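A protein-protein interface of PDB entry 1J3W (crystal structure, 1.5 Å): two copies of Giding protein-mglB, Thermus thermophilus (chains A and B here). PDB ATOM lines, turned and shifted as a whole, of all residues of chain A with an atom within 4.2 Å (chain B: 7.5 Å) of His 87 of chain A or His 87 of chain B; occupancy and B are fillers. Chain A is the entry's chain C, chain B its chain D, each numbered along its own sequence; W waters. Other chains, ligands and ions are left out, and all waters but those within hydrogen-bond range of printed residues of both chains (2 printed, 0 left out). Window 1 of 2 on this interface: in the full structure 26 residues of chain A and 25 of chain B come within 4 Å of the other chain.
Among the printed residues, pairs that only touch across the chains: Val 86 of chain A with Glu 85 of chain B, Glu 85 of chain A with Val 86 of chain B, Asn 66 of chain A with Thr 70 of chain B, Thr 70 of chain A with Asn 66 of chain B, Phe 82 of chain A with Gln 88 of chain B, His 87 of chain A with Phe 82 of chain B, Phe 82 of chain A with His 87 of chain B, Gln 88 of chain A with Phe 82 of chain B, His 87 of chain A with Glu 84 of chain B, Glu 84 of chain A with His 87 of chain B, Thr 70 of chain A with His 87 of chain B, Phe 82 of chain A with Gly 89 of chain B, His 87 of chain A with His 87 of chain B, His 87 of chain A with Thr 70 of chain B, Asn 66 of chain A with Asn 66 of chain B and Asn 66 of chain A with Leu 73 of chain B.
The side-chain hydroxyl of Thr 70 of chain A lies within hydrogen-bond range of the side-chain carboxylate of Glu 85 of chain A, 2.9 Å away.
N of Leu 94 of chain A sits at hydrogen-bond distance from O of His 87 of chain A (2.8 Å).
ND2 of Asn 66 of chain B lies within hydrogen-bond range of OE2 of Glu 85 of chain B.
The side-chain carboxylate (OE1) of Glu 85 of chain B is in hydrogen-bond range of the side-chain hydroxyl (OG1) of Thr 70 of chain B, 3.0 Å away.
The side-chain carboxylate of Glu 84 of chain B is in hydrogen-bond range of the side-chain hydroxyl of Tyr 95 of chain B.
The side-chain amide nitrogen (NE2) of Gln 88 of chain B sits at hydrogen-bond distance from the backbone carbonyl oxygen (O) of Met 92 of chain B.
Of chain B, only Thr 70, Phe 82, Glu 84, Glu 85 and His 87 come within 4 Å of His 87 of chain A.
His 87 of chain B touches just these residues of chain A: Thr 70 (3.8 Å), Phe 82 (3.7 Å), Glu 84 (3.7 Å), Glu 85 (3.1 Å) and His 87 (3.9 Å).
Of the printed residues of chain B, Asn 66 of chain A touches Asn 66 (3.97 Å), Thr 70 (3.5 Å) and Leu 73 (3.99 Å).
Of the printed residues of chain A, Asn 66 of chain B touches Asn 66 (3.97 Å) and Thr 70 (3.6 Å).
Of the printed residues of chain B, Gln 88 of chain A touches Phe 82, Gln 83 and Glu 84.
Of the printed residues of chain A, Glu 84 of chain B touches His 87 (3.7 Å) and Gln 88 (2.8 Å).
Met 92 of chain B touches none of the printed residues of chain A.
Leu 77 of chain B touches none of the printed residues of chain A.
The nearest printed residue of chain B that does not touch His 87 of chain A is Val 86 of chain B (5.1 Å).
The nearest printed residue of chain A that does not touch Gln 88 of chain B is Glu 85 of chain A (4.9 Å).
Of the 10 printed residues of chain A, 8 touch a printed residue of chain B.
Hydrophobic or aromatic side chains of chain A that line the printed part of chain B: Phe 82 and His 87.
Hydrophobic or aromatic side chains of chain B within 4 Å of the printed part of chain A: Leu 73, Phe 82 and His 87.
Along chain B the printed residues that touch a printed residue of chain A span positions 66 to 89.
The backbone carbonyl oxygen (O) of Glu 84 of chain A is in hydrogen-bond range of the backbone NH (N) of Gln 88 of chain B (2.8 Å).
The side-chain carboxylate of Glu 85 of chain A lies close to a ring nitrogen (NE2) of His 87 of chain B (3.3 Å).
O of Val 86 of chain A lies within hydrogen-bond range of N of Val 86 of chain B (2.9 Å).
The side-chain carboxylate (OE2) of Glu 85 of chain B sits close to a ring nitrogen (NE2) of His 87 of chain A, at 3.5 Å.
The backbone NH (N) of Gln 83 of chain B lies within hydrogen-bond range of the backbone carbonyl oxygen (O) of Gln 88 of chain A (2.9 Å).
O of Glu 84 of chain B is in hydrogen-bond range of N of Gln 88 of chain A, at 2.8 Å.
Water W1 lies within hydrogen-bond range of the side-chain amide oxygen (OD1) of Asn 66 of chain B, the side-chain amide oxygen (OD1) of Asn 66 of chain A, a ring nitrogen (NE2) of His 87 of chain B and a ring nitrogen (NE2) of His 87 of chain A.
Water W2 lies within hydrogen-bond range of the side-chain carboxylate of Glu 84 of chain A (2.7 Å) and the side-chain amide oxygen of Gln 88 of chain B (3.3 Å).
Asn 66 of chain B touches its own counterpart, Asn 66 of chain A.
Phe 82 of chain A touches Gln 88 of chain B, and with the chains exchanged Gln 88 of chain A touches Phe 82 of chain B.
Glu 84 of chain A touches His 87 of chain B, and with the chains exchanged His 87 of chain A touches Glu 84 of chain B.
Glu 84 of chain A touches Gln 88 of chain B, and with the chains exchanged Gln 88 of chain A touches Glu 84 of chain B.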
ATOM      1  N   ASN A  66      -7.961  11.783  13.844  1.00  0.00           N
ATOM      2  CA  ASN A  66      -7.455  12.415  12.633  1.00  0.00           C
ATOM      3  C   ASN A  66      -6.414  13.473  12.982  1.00  0.00           C
ATOM      4  O   ASN A  66      -5.382  13.578  12.319  1.00  0.00           O
ATOM      5  CB  ASN A  66      -8.600  13.074  11.863  1.00  0.00           C
ATOM      6  CG  ASN A  66      -8.120  13.778  10.612  1.00  0.00           C
ATOM      7  OD1 ASN A  66      -7.827  13.141   9.606  1.00  0.00           O
ATOM      8  ND2 ASN A  66      -8.025  15.104  10.676  1.00  0.00           N
ATOM      9  N   THR A  70      -2.622  13.229  11.181  1.00  0.00           N
ATOM     10  CA  THR A  70      -2.081  14.141  10.176  1.00  0.00           C
ATOM     11  C   THR A  70      -0.802  14.863  10.582  1.00  0.00           C
ATOM     12  O   THR A  70      -0.243  15.619   9.790  1.00  0.00           O
ATOM     13  CB  THR A  70      -3.116  15.209   9.767  1.00  0.00           C
ATOM     14  OG1 THR A  70      -3.454  16.007  10.906  1.00  0.00           O
ATOM     15  CG2 THR A  70      -4.376  14.550   9.205  1.00  0.00           C
ATOM     16  N   PHE A  82      -1.164  20.622  11.582  1.00  0.00           N
ATOM     17  CA  PHE A  82      -2.057  21.474  10.807  1.00  0.00           C
ATOM     18  C   PHE A  82      -3.038  22.112  11.772  1.00  0.00           C
ATOM     19  O   PHE A  82      -3.703  21.415  12.539  1.00  0.00           O
ATOM     20  CB  PHE A  82      -2.829  20.655   9.770  1.00  0.00           C
ATOM     21  CG  PHE A  82      -1.965  20.067   8.697  1.00  0.00           C
ATOM     22  CD1 PHE A  82      -1.240  20.892   7.843  1.00  0.00           C
ATOM     23  CD2 PHE A  82      -1.868  18.689   8.540  1.00  0.00           C
ATOM     24  CE1 PHE A  82      -0.431  20.358   6.847  1.00  0.00           C
ATOM     25  CE2 PHE A  82      -1.064  18.140   7.549  1.00  0.00           C
ATOM     26  CZ  PHE A  82      -0.342  18.979   6.698  1.00  0.00           C
ATOM     27  N   GLU A  84      -5.635  24.120  10.801  1.00  0.00           N
ATOM     28  CA  GLU A  84      -6.959  24.129  10.193  1.00  0.00           C
ATOM     29  C   GLU A  84      -7.079  23.057   9.118  1.00  0.00           C
ATOM     30  O   GLU A  84      -6.153  22.848   8.336  1.00  0.00           O
ATOM     31  CB  GLU A  84      -7.224  25.509   9.586  1.00  0.00           C
ATOM     32  CG  GLU A  84      -8.586  25.700   8.949  1.00  0.00           C
ATOM     33  CD  GLU A  84      -8.712  27.062   8.282  1.00  0.00           C
ATOM     34  OE1 GLU A  84      -7.938  27.337   7.339  1.00  0.00           O
ATOM     35  OE2 GLU A  84      -9.577  27.858   8.702  1.00  0.00           O
ATOM     36  N   GLU A  85      -8.222  22.381   9.083  1.00  0.00           N
ATOM     37  CA  GLU A  85      -8.460  21.334   8.097  1.00  0.00           C
ATOM     38  C   GLU A  85      -9.902  21.367   7.613  1.00  0.00           C
ATOM     39  O   GLU A  85     -10.823  21.591   8.396  1.00  0.00           O
ATOM     40  CB  GLU A  85      -8.178  19.950   8.697  1.00  0.00           C
ATOM     41  CG  GLU A  85      -6.709  19.656   8.982  1.00  0.00           C
ATOM     42  CD  GLU A  85      -6.486  18.244   9.498  1.00  0.00           C
ATOM     43  OE1 GLU A  85      -7.287  17.349   9.150  1.00  0.00           O
ATOM     44  OE2 GLU A  85      -5.501  18.021  10.234  1.00  0.00           O
ATOM     45  N   VAL A  86     -10.089  21.139   6.318  1.00  0.00           N
ATOM     46  CA  VAL A  86     -11.414  21.099   5.721  1.00  0.00           C
ATOM     47  C   VAL A  86     -11.533  19.827   4.887  1.00  0.00           C
ATOM     48  O   VAL A  86     -10.690  19.553   4.030  1.00  0.00           O
ATOM     49  CB  VAL A  86     -11.673  22.326   4.812  1.00  0.00           C
ATOM     50  CG1 VAL A  86     -13.002  22.170   4.088  1.00  0.00           C
ATOM     51  CG2 VAL A  86     -11.682  23.594   5.651  1.00  0.00           C
ATOM     52  N   HIS A  87     -12.568  19.042   5.164  1.00  0.00           N
ATOM     53  CA  HIS A  87     -12.821  17.804   4.438  1.00  0.00           C
ATOM     54  C   HIS A  87     -14.191  17.953   3.801  1.00  0.00           C
ATOM     55  O   HIS A  87     -15.176  18.202   4.495  1.00  0.00           O
ATOM     56  CB  HIS A  87     -12.828  16.607   5.391  1.00  0.00           C
ATOM     57  CG  HIS A  87     -11.497  16.311   6.008  1.00  0.00           C
ATOM     58  ND1 HIS A  87     -10.943  17.087   7.001  1.00  0.00           N
ATOM     59  CD2 HIS A  87     -10.608  15.317   5.768  1.00  0.00           C
ATOM     60  CE1 HIS A  87      -9.772  16.585   7.349  1.00  0.00           C
ATOM     61  NE2 HIS A  87      -9.545  15.511   6.616  1.00  0.00           N
ATOM     62  N   GLN A  88     -14.262  17.794   2.485  1.00  0.00           N
ATOM     63  CA  GLN A  88     -15.525  17.953   1.781  1.00  0.00           C
ATOM     64  C   GLN A  88     -15.914  16.738   0.953  1.00  0.00           C
ATOM     65  O   GLN A  88     -15.115  16.227   0.172  1.00  0.00           O
ATOM     66  CB  GLN A  88     -15.448  19.188   0.876  1.00  0.00           C
ATOM     67  CG  GLN A  88     -16.683  19.445   0.021  1.00  0.00           C
ATOM     68  CD  GLN A  88     -17.913  19.790   0.841  1.00  0.00           C
ATOM     69  OE1 GLN A  88     -17.883  20.693   1.678  1.00  0.00           O
ATOM     70  NE2 GLN A  88     -19.007  19.078   0.595  1.00  0.00           N
ATOM     71  N   GLY A  93     -19.663  18.661   4.642  1.00  0.00           N
ATOM     72  CA  GLY A  93     -18.326  19.183   4.851  1.00  0.00           C
ATOM     73  C   GLY A  93     -17.975  19.198   6.325  1.00  0.00           C
ATOM     74  O   GLY A  93     -18.853  19.269   7.188  1.00  0.00           O
ATOM     75  N   LEU A  94     -16.679  19.119   6.610  1.00  0.00           N
ATOM     76  CA  LEU A  94     -16.178  19.120   7.974  1.00  0.00           C
ATOM     77  C   LEU A  94     -15.061  20.147   8.106  1.00  0.00           C
ATOM     78  O   LEU A  94     -14.102  20.138   7.331  1.00  0.00           O
ATOM     79  CB  LEU A  94     -15.644  17.726   8.323  1.00  0.00           C
ATOM     80  CG  LEU A  94     -15.029  17.501   9.704  1.00  0.00           C
ATOM     81  CD1 LEU A  94     -16.107  17.552  10.772  1.00  0.00           C
ATOM     82  CD2 LEU A  94     -14.339  16.142   9.720  1.00  0.00           C
ATOM     83  N   ASN B  66      -3.502   8.809   4.786  1.00  0.00           N
ATOM     84  CA  ASN B  66      -4.561   9.712   5.215  1.00  0.00           C
ATOM     85  C   ASN B  66      -5.857   9.423   4.464  1.00  0.00           C
ATOM     86  O   ASN B  66      -6.938   9.419   5.057  1.00  0.00           O
ATOM     87  CB  ASN B  66      -4.142  11.161   4.957  1.00  0.00           C
ATOM     88  CG  ASN B  66      -5.222  12.156   5.340  1.00  0.00           C
ATOM     89  OD1 ASN B  66      -5.446  12.418   6.518  1.00  0.00           O
ATOM     90  ND2 ASN B  66      -5.907  12.707   4.340  1.00  0.00           N
ATOM     91  N   THR B  70      -9.259   8.731   6.729  1.00  0.00           N
ATOM     92  CA  THR B  70     -10.393   9.646   6.828  1.00  0.00           C
ATOM     93  C   THR B  70     -11.732   9.082   6.369  1.00  0.00           C
ATOM     94  O   THR B  70     -12.762   9.733   6.527  1.00  0.00           O
ATOM     95  CB  THR B  70     -10.135  10.959   6.058  1.00  0.00           C
ATOM     96  OG1 THR B  70      -9.989  10.680   4.661  1.00  0.00           O
ATOM     97  CG2 THR B  70      -8.875  11.640   6.576  1.00  0.00           C
ATOM     98  N   LEU B  73     -14.448   8.882   9.155  1.00  0.00           N
ATOM     99  CA  LEU B  73     -15.118  10.157   9.398  1.00  0.00           C
ATOM    100  C   LEU B  73     -16.126  10.434   8.287  1.00  0.00           C
ATOM    101  O   LEU B  73     -17.242  10.881   8.547  1.00  0.00           O
ATOM    102  CB  LEU B  73     -14.103  11.305   9.427  1.00  0.00           C
ATOM    103  CG  LEU B  73     -13.458  11.689  10.757  1.00  0.00           C
ATOM    104  CD1 LEU B  73     -12.331  12.679  10.497  1.00  0.00           C
ATOM    105  CD2 LEU B  73     -14.505  12.291  11.689  1.00  0.00           C
ATOM    106  N   ALA B  74     -15.728  10.169   7.049  1.00  0.00           N
ATOM    107  CA  ALA B  74     -16.600  10.404   5.906  1.00  0.00           C
ATOM    108  C   ALA B  74     -17.910   9.639   6.042  1.00  0.00           C
ATOM    109  O   ALA B  74     -18.992  10.201   5.872  1.00  0.00           O
ATOM    110  CB  ALA B  74     -15.894  10.002   4.622  1.00  0.00           C
ATOM    111  N   LEU B  77     -20.460  10.888   8.337  1.00  0.00           N
ATOM    112  CA  LEU B  77     -21.137  12.062   7.787  1.00  0.00           C
ATOM    113  C   LEU B  77     -21.973  11.731   6.547  1.00  0.00           C
ATOM    114  O   LEU B  77     -22.405  12.628   5.820  1.00  0.00           O
ATOM    115  CB  LEU B  77     -20.114  13.154   7.450  1.00  0.00           C
ATOM    116  CG  LEU B  77     -19.302  13.697   8.632  1.00  0.00           C
ATOM    117  CD1 LEU B  77     -18.352  14.780   8.143  1.00  0.00           C
ATOM    118  CD2 LEU B  77     -20.235  14.255   9.698  1.00  0.00           C
ATOM    119  N   PHE B  82     -14.141  11.432   1.472  1.00  0.00           N
ATOM    120  CA  PHE B  82     -14.029  12.845   1.141  1.00  0.00           C
ATOM    121  C   PHE B  82     -13.397  12.975  -0.232  1.00  0.00           C
ATOM    122  O   PHE B  82     -12.395  12.324  -0.529  1.00  0.00           O
ATOM    123  CB  PHE B  82     -13.180  13.564   2.187  1.00  0.00           C
ATOM    124  CG  PHE B  82     -13.816  13.605   3.546  1.00  0.00           C
ATOM    125  CD1 PHE B  82     -15.031  14.256   3.737  1.00  0.00           C
ATOM    126  CD2 PHE B  82     -13.207  12.990   4.637  1.00  0.00           C
ATOM    127  CE1 PHE B  82     -15.632  14.296   4.995  1.00  0.00           C
ATOM    128  CE2 PHE B  82     -13.800  13.024   5.898  1.00  0.00           C
ATOM    129  CZ  PHE B  82     -15.016  13.679   6.078  1.00  0.00           C
ATOM    130  N   GLN B  83     -13.986  13.810  -1.075  1.00  0.00           N
ATOM    131  CA  GLN B  83     -13.457  13.997  -2.419  1.00  0.00           C
ATOM    132  C   GLN B  83     -12.374  15.065  -2.446  1.00  0.00           C
ATOM    133  O   GLN B  83     -11.454  15.007  -3.260  1.00  0.00           O
ATOM    134  CB  GLN B  83     -14.587  14.383  -3.375  1.00  0.00           C
ATOM    135  CG  GLN B  83     -15.333  15.642  -2.974  1.00  0.00           C
ATOM    136  CD  GLN B  83     -16.493  15.954  -3.902  1.00  0.00           C
ATOM    137  OE1 GLN B  83     -17.396  15.137  -4.080  1.00  0.00           O
ATOM    138  NE2 GLN B  83     -16.475  17.143  -4.495  1.00  0.00           N
ATOM    139  N   GLU B  84     -12.481  16.028  -1.536  1.00  0.00           N
ATOM    140  CA  GLU B  84     -11.533  17.131  -1.473  1.00  0.00           C
ATOM    141  C   GLU B  84     -11.135  17.413  -0.029  1.00  0.00           C
ATOM    142  O   GLU B  84     -11.983  17.412   0.865  1.00  0.00           O
ATOM    143  CB  GLU B  84     -12.186  18.368  -2.097  1.00  0.00           C
ATOM    144  CG  GLU B  84     -11.351  19.627  -2.111  1.00  0.00           C
ATOM    145  CD  GLU B  84     -12.096  20.787  -2.750  1.00  0.00           C
ATOM    146  OE1 GLU B  84     -13.209  21.106  -2.283  1.00  0.00           O
ATOM    147  OE2 GLU B  84     -11.573  21.378  -3.719  1.00  0.00           O
ATOM    148  N   GLU B  85      -9.846  17.645   0.201  1.00  0.00           N
ATOM    149  CA  GLU B  85      -9.356  17.937   1.543  1.00  0.00           C
ATOM    150  C   GLU B  85      -8.276  19.008   1.506  1.00  0.00           C
ATOM    151  O   GLU B  85      -7.424  19.017   0.616  1.00  0.00           O
ATOM    152  CB  GLU B  85      -8.765  16.682   2.201  1.00  0.00           C
ATOM    153  CG  GLU B  85      -9.722  15.510   2.375  1.00  0.00           C
ATOM    154  CD  GLU B  85      -9.106  14.373   3.180  1.00  0.00           C
ATOM    155  OE1 GLU B  85      -9.763  13.320   3.331  1.00  0.00           O
ATOM    156  OE2 GLU B  85      -7.966  14.533   3.673  1.00  0.00           O
ATOM    157  N   VAL B  86      -8.316  19.912   2.477  1.00  0.00           N
ATOM    158  CA  VAL B  86      -7.309  20.960   2.584  1.00  0.00           C
ATOM    159  C   VAL B  86      -6.775  20.954   4.008  1.00  0.00           C
ATOM    160  O   VAL B  86      -7.545  20.986   4.967  1.00  0.00           O
ATOM    161  CB  VAL B  86      -7.888  22.364   2.288  1.00  0.00           C
ATOM    162  CG1 VAL B  86      -6.834  23.430   2.570  1.00  0.00           C
ATOM    163  CG2 VAL B  86      -8.335  22.447   0.839  1.00  0.00           C
ATOM    164  N   HIS B  87      -5.457  20.882   4.136  1.00  0.00           N
ATOM    165  CA  HIS B  87      -4.804  20.904   5.438  1.00  0.00           C
ATOM    166  C   HIS B  87      -3.936  22.151   5.437  1.00  0.00           C
ATOM    167  O   HIS B  87      -3.105  22.332   4.545  1.00  0.00           O
ATOM    168  CB  HIS B  87      -3.938  19.657   5.632  1.00  0.00           C
ATOM    169  CG  HIS B  87      -4.723  18.387   5.730  1.00  0.00           C
ATOM    170  ND1 HIS B  87      -5.316  17.789   4.639  1.00  0.00           N
ATOM    171  CD2 HIS B  87      -5.038  17.616   6.797  1.00  0.00           C
ATOM    172  CE1 HIS B  87      -5.963  16.706   5.030  1.00  0.00           C
ATOM    173  NE2 HIS B  87      -5.810  16.580   6.336  1.00  0.00           N
ATOM    174  N   GLN B  88      -4.125  23.007   6.433  1.00  0.00           N
ATOM    175  CA  GLN B  88      -3.380  24.258   6.496  1.00  0.00           C
ATOM    176  C   GLN B  88      -2.554  24.442   7.759  1.00  0.00           C
ATOM    177  O   GLN B  88      -3.075  24.353   8.873  1.00  0.00           O
ATOM    178  CB  GLN B  88      -4.358  25.430   6.366  1.00  0.00           C
ATOM    179  CG  GLN B  88      -3.702  26.799   6.369  1.00  0.00           C
ATOM    180  CD  GLN B  88      -3.014  27.110   5.060  1.00  0.00           C
ATOM    181  OE1 GLN B  88      -3.664  27.214   4.019  1.00  0.00           O
ATOM    182  NE2 GLN B  88      -1.694  27.254   5.101  1.00  0.00           N
ATOM    183  N   GLY B  89      -1.264  24.701   7.569  1.00  0.00           N
ATOM    184  CA  GLY B  89      -0.369  24.941   8.686  1.00  0.00           C
ATOM    185  C   GLY B  89      -0.121  26.440   8.762  1.00  0.00           C
ATOM    186  O   GLY B  89      -0.857  27.216   8.160  1.00  0.00           O
ATOM    187  N   MET B  92       2.775  26.310   5.406  1.00  0.00           N
ATOM    188  CA  MET B  92       2.536  25.310   4.373  1.00  0.00           C
ATOM    189  C   MET B  92       1.122  24.749   4.374  1.00  0.00           C
ATOM    190  O   MET B  92       0.487  24.630   5.423  1.00  0.00           O
ATOM    191  CB  MET B  92       3.530  24.158   4.525  1.00  0.00           C
ATOM    192  CG  MET B  92       4.984  24.555   4.342  1.00  0.00           C
ATOM    193  SD  MET B  92       5.311  25.203   2.690  1.00  0.00           S
ATOM    194  CE  MET B  92       5.529  23.688   1.766  1.00  0.00           C
ATOM    195  N   GLY B  93       0.649  24.398   3.182  1.00  0.00           N
ATOM    196  CA  GLY B  93      -0.681  23.839   3.026  1.00  0.00           C
ATOM    197  C   GLY B  93      -0.668  22.661   2.072  1.00  0.00           C
ATOM    198  O   GLY B  93       0.247  22.506   1.255  1.00  0.00           O
ATOM    199  N   LEU B  94      -1.701  21.832   2.168  1.00  0.00           N
ATOM    200  CA  LEU B  94      -1.828  20.648   1.335  1.00  0.00           C
ATOM    201  C   LEU B  94      -3.254  20.528   0.807  1.00  0.00           C
ATOM    202  O   LEU B  94      -4.215  20.631   1.571  1.00  0.00           O
ATOM    203  CB  LEU B  94      -1.486  19.404   2.164  1.00  0.00           C
ATOM    204  CG  LEU B  94      -1.539  18.037   1.482  1.00  0.00           C
ATOM    205  CD1 LEU B  94      -0.348  17.891   0.547  1.00  0.00           C
ATOM    206  CD2 LEU B  94      -1.509  16.941   2.539  1.00  0.00           C
ATOM    207  N   TYR B  95      -3.383  20.320  -0.499  1.00  0.00           N
ATOM    208  CA  TYR B  95      -4.680  20.156  -1.143  1.00  0.00           C
ATOM    209  C   TYR B  95      -4.700  18.778  -1.794  1.00  0.00           C
ATOM    210  O   TYR B  95      -3.786  18.428  -2.540  1.00  0.00           O
ATOM    211  CB  TYR B  95      -4.887  21.226  -2.221  1.00  0.00           C
ATOM    212  CG  TYR B  95      -6.144  21.034  -3.047  1.00  0.00           C
ATOM    213  CD1 TYR B  95      -7.395  21.387  -2.544  1.00  0.00           C
ATOM    214  CD2 TYR B  95      -6.081  20.477  -4.323  1.00  0.00           C
ATOM    215  CE1 TYR B  95      -8.557  21.188  -3.296  1.00  0.00           C
ATOM    216  CE2 TYR B  95      -7.236  20.277  -5.083  1.00  0.00           C
ATOM    217  CZ  TYR B  95      -8.468  20.633  -4.564  1.00  0.00           C
ATOM    218  OH  TYR B  95      -9.612  20.431  -5.305  1.00  0.00           O
ATOM    219  N   VAL B  96      -5.728  17.990  -1.502  1.00  0.00           N
ATOM    220  CA  VAL B  96      -5.845  16.659  -2.088  1.00  0.00           C
ATOM    221  C   VAL B  96      -7.243  16.504  -2.659  1.00  0.00           C
ATOM    222  O   VAL B  96      -8.231  16.783  -1.981  1.00  0.00           O
ATOM    223  CB  VAL B  96      -5.604  15.551  -1.041  1.00  0.00           C
ATOM    224  CG1 VAL B  96      -5.678  14.180  -1.713  1.00  0.00           C
ATOM    225  CG2 VAL B  96      -4.246  15.741  -0.388  1.00  0.00           C
ATOM    226  N   LEU B 107      -1.500  18.813  -4.211  1.00  0.00           N
ATOM    227  CA  LEU B 107      -0.853  20.099  -4.433  1.00  0.00           C
ATOM    228  C   LEU B 107      -0.333  20.593  -3.092  1.00  0.00           C
ATOM    229  O   LEU B 107      -1.090  20.699  -2.123  1.00  0.00           O
ATOM    230  CB  LEU B 107      -1.834  21.128  -5.008  1.00  0.00           C
ATOM    231  CG  LEU B 107      -2.383  20.898  -6.421  1.00  0.00           C
ATOM    232  CD1 LEU B 107      -3.343  22.026  -6.785  1.00  0.00           C
ATOM    233  CD2 LEU B 107      -1.237  20.843  -7.424  1.00  0.00           C
ATOM    234  N   PHE B 109       1.409  23.730  -1.195  1.00  0.00           N
ATOM    235  CA  PHE B 109       1.552  25.160  -1.419  1.00  0.00           C
ATOM    236  C   PHE B 109       1.943  25.930  -0.169  1.00  0.00           C
ATOM    237  O   PHE B 109       1.864  25.417   0.944  1.00  0.00           O
ATOM    238  CB  PHE B 109       0.240  25.709  -1.985  1.00  0.00           C
ATOM    239  CG  PHE B 109      -0.950  25.484  -1.090  1.00  0.00           C
ATOM    240  CD1 PHE B 109      -1.305  26.425  -0.129  1.00  0.00           C
ATOM    241  CD2 PHE B 109      -1.714  24.325  -1.203  1.00  0.00           C
ATOM    242  CE1 PHE B 109      -2.404  26.218   0.705  1.00  0.00           C
ATOM    243  CE2 PHE B 109      -2.813  24.108  -0.376  1.00  0.00           C
ATOM    244  CZ  PHE B 109      -3.161  25.054   0.581  1.00  0.00           C
ATOM    245  N   LEU B 115      -5.359  30.291  -2.195  1.00  0.00           N
ATOM    246  CA  LEU B 115      -6.155  29.087  -1.970  1.00  0.00           C
ATOM    247  C   LEU B 115      -7.331  28.959  -2.930  1.00  0.00           C
ATOM    248  O   LEU B 115      -7.659  27.860  -3.366  1.00  0.00           O
ATOM    249  CB  LEU B 115      -6.662  29.042  -0.527  1.00  0.00           C
ATOM    250  CG  LEU B 115      -7.434  27.775  -0.144  1.00  0.00           C
ATOM    251  CD1 LEU B 115      -6.542  26.548  -0.301  1.00  0.00           C
ATOM    252  CD2 LEU B 115      -7.920  27.895   1.293  1.00  0.00           C
HETATM  253  O   HOH W   1      -7.094  14.274   7.250  1.00  0.00           O
HETATM  254  O   HOH W   2      -6.804  26.990   4.889  1.00  0.00           O
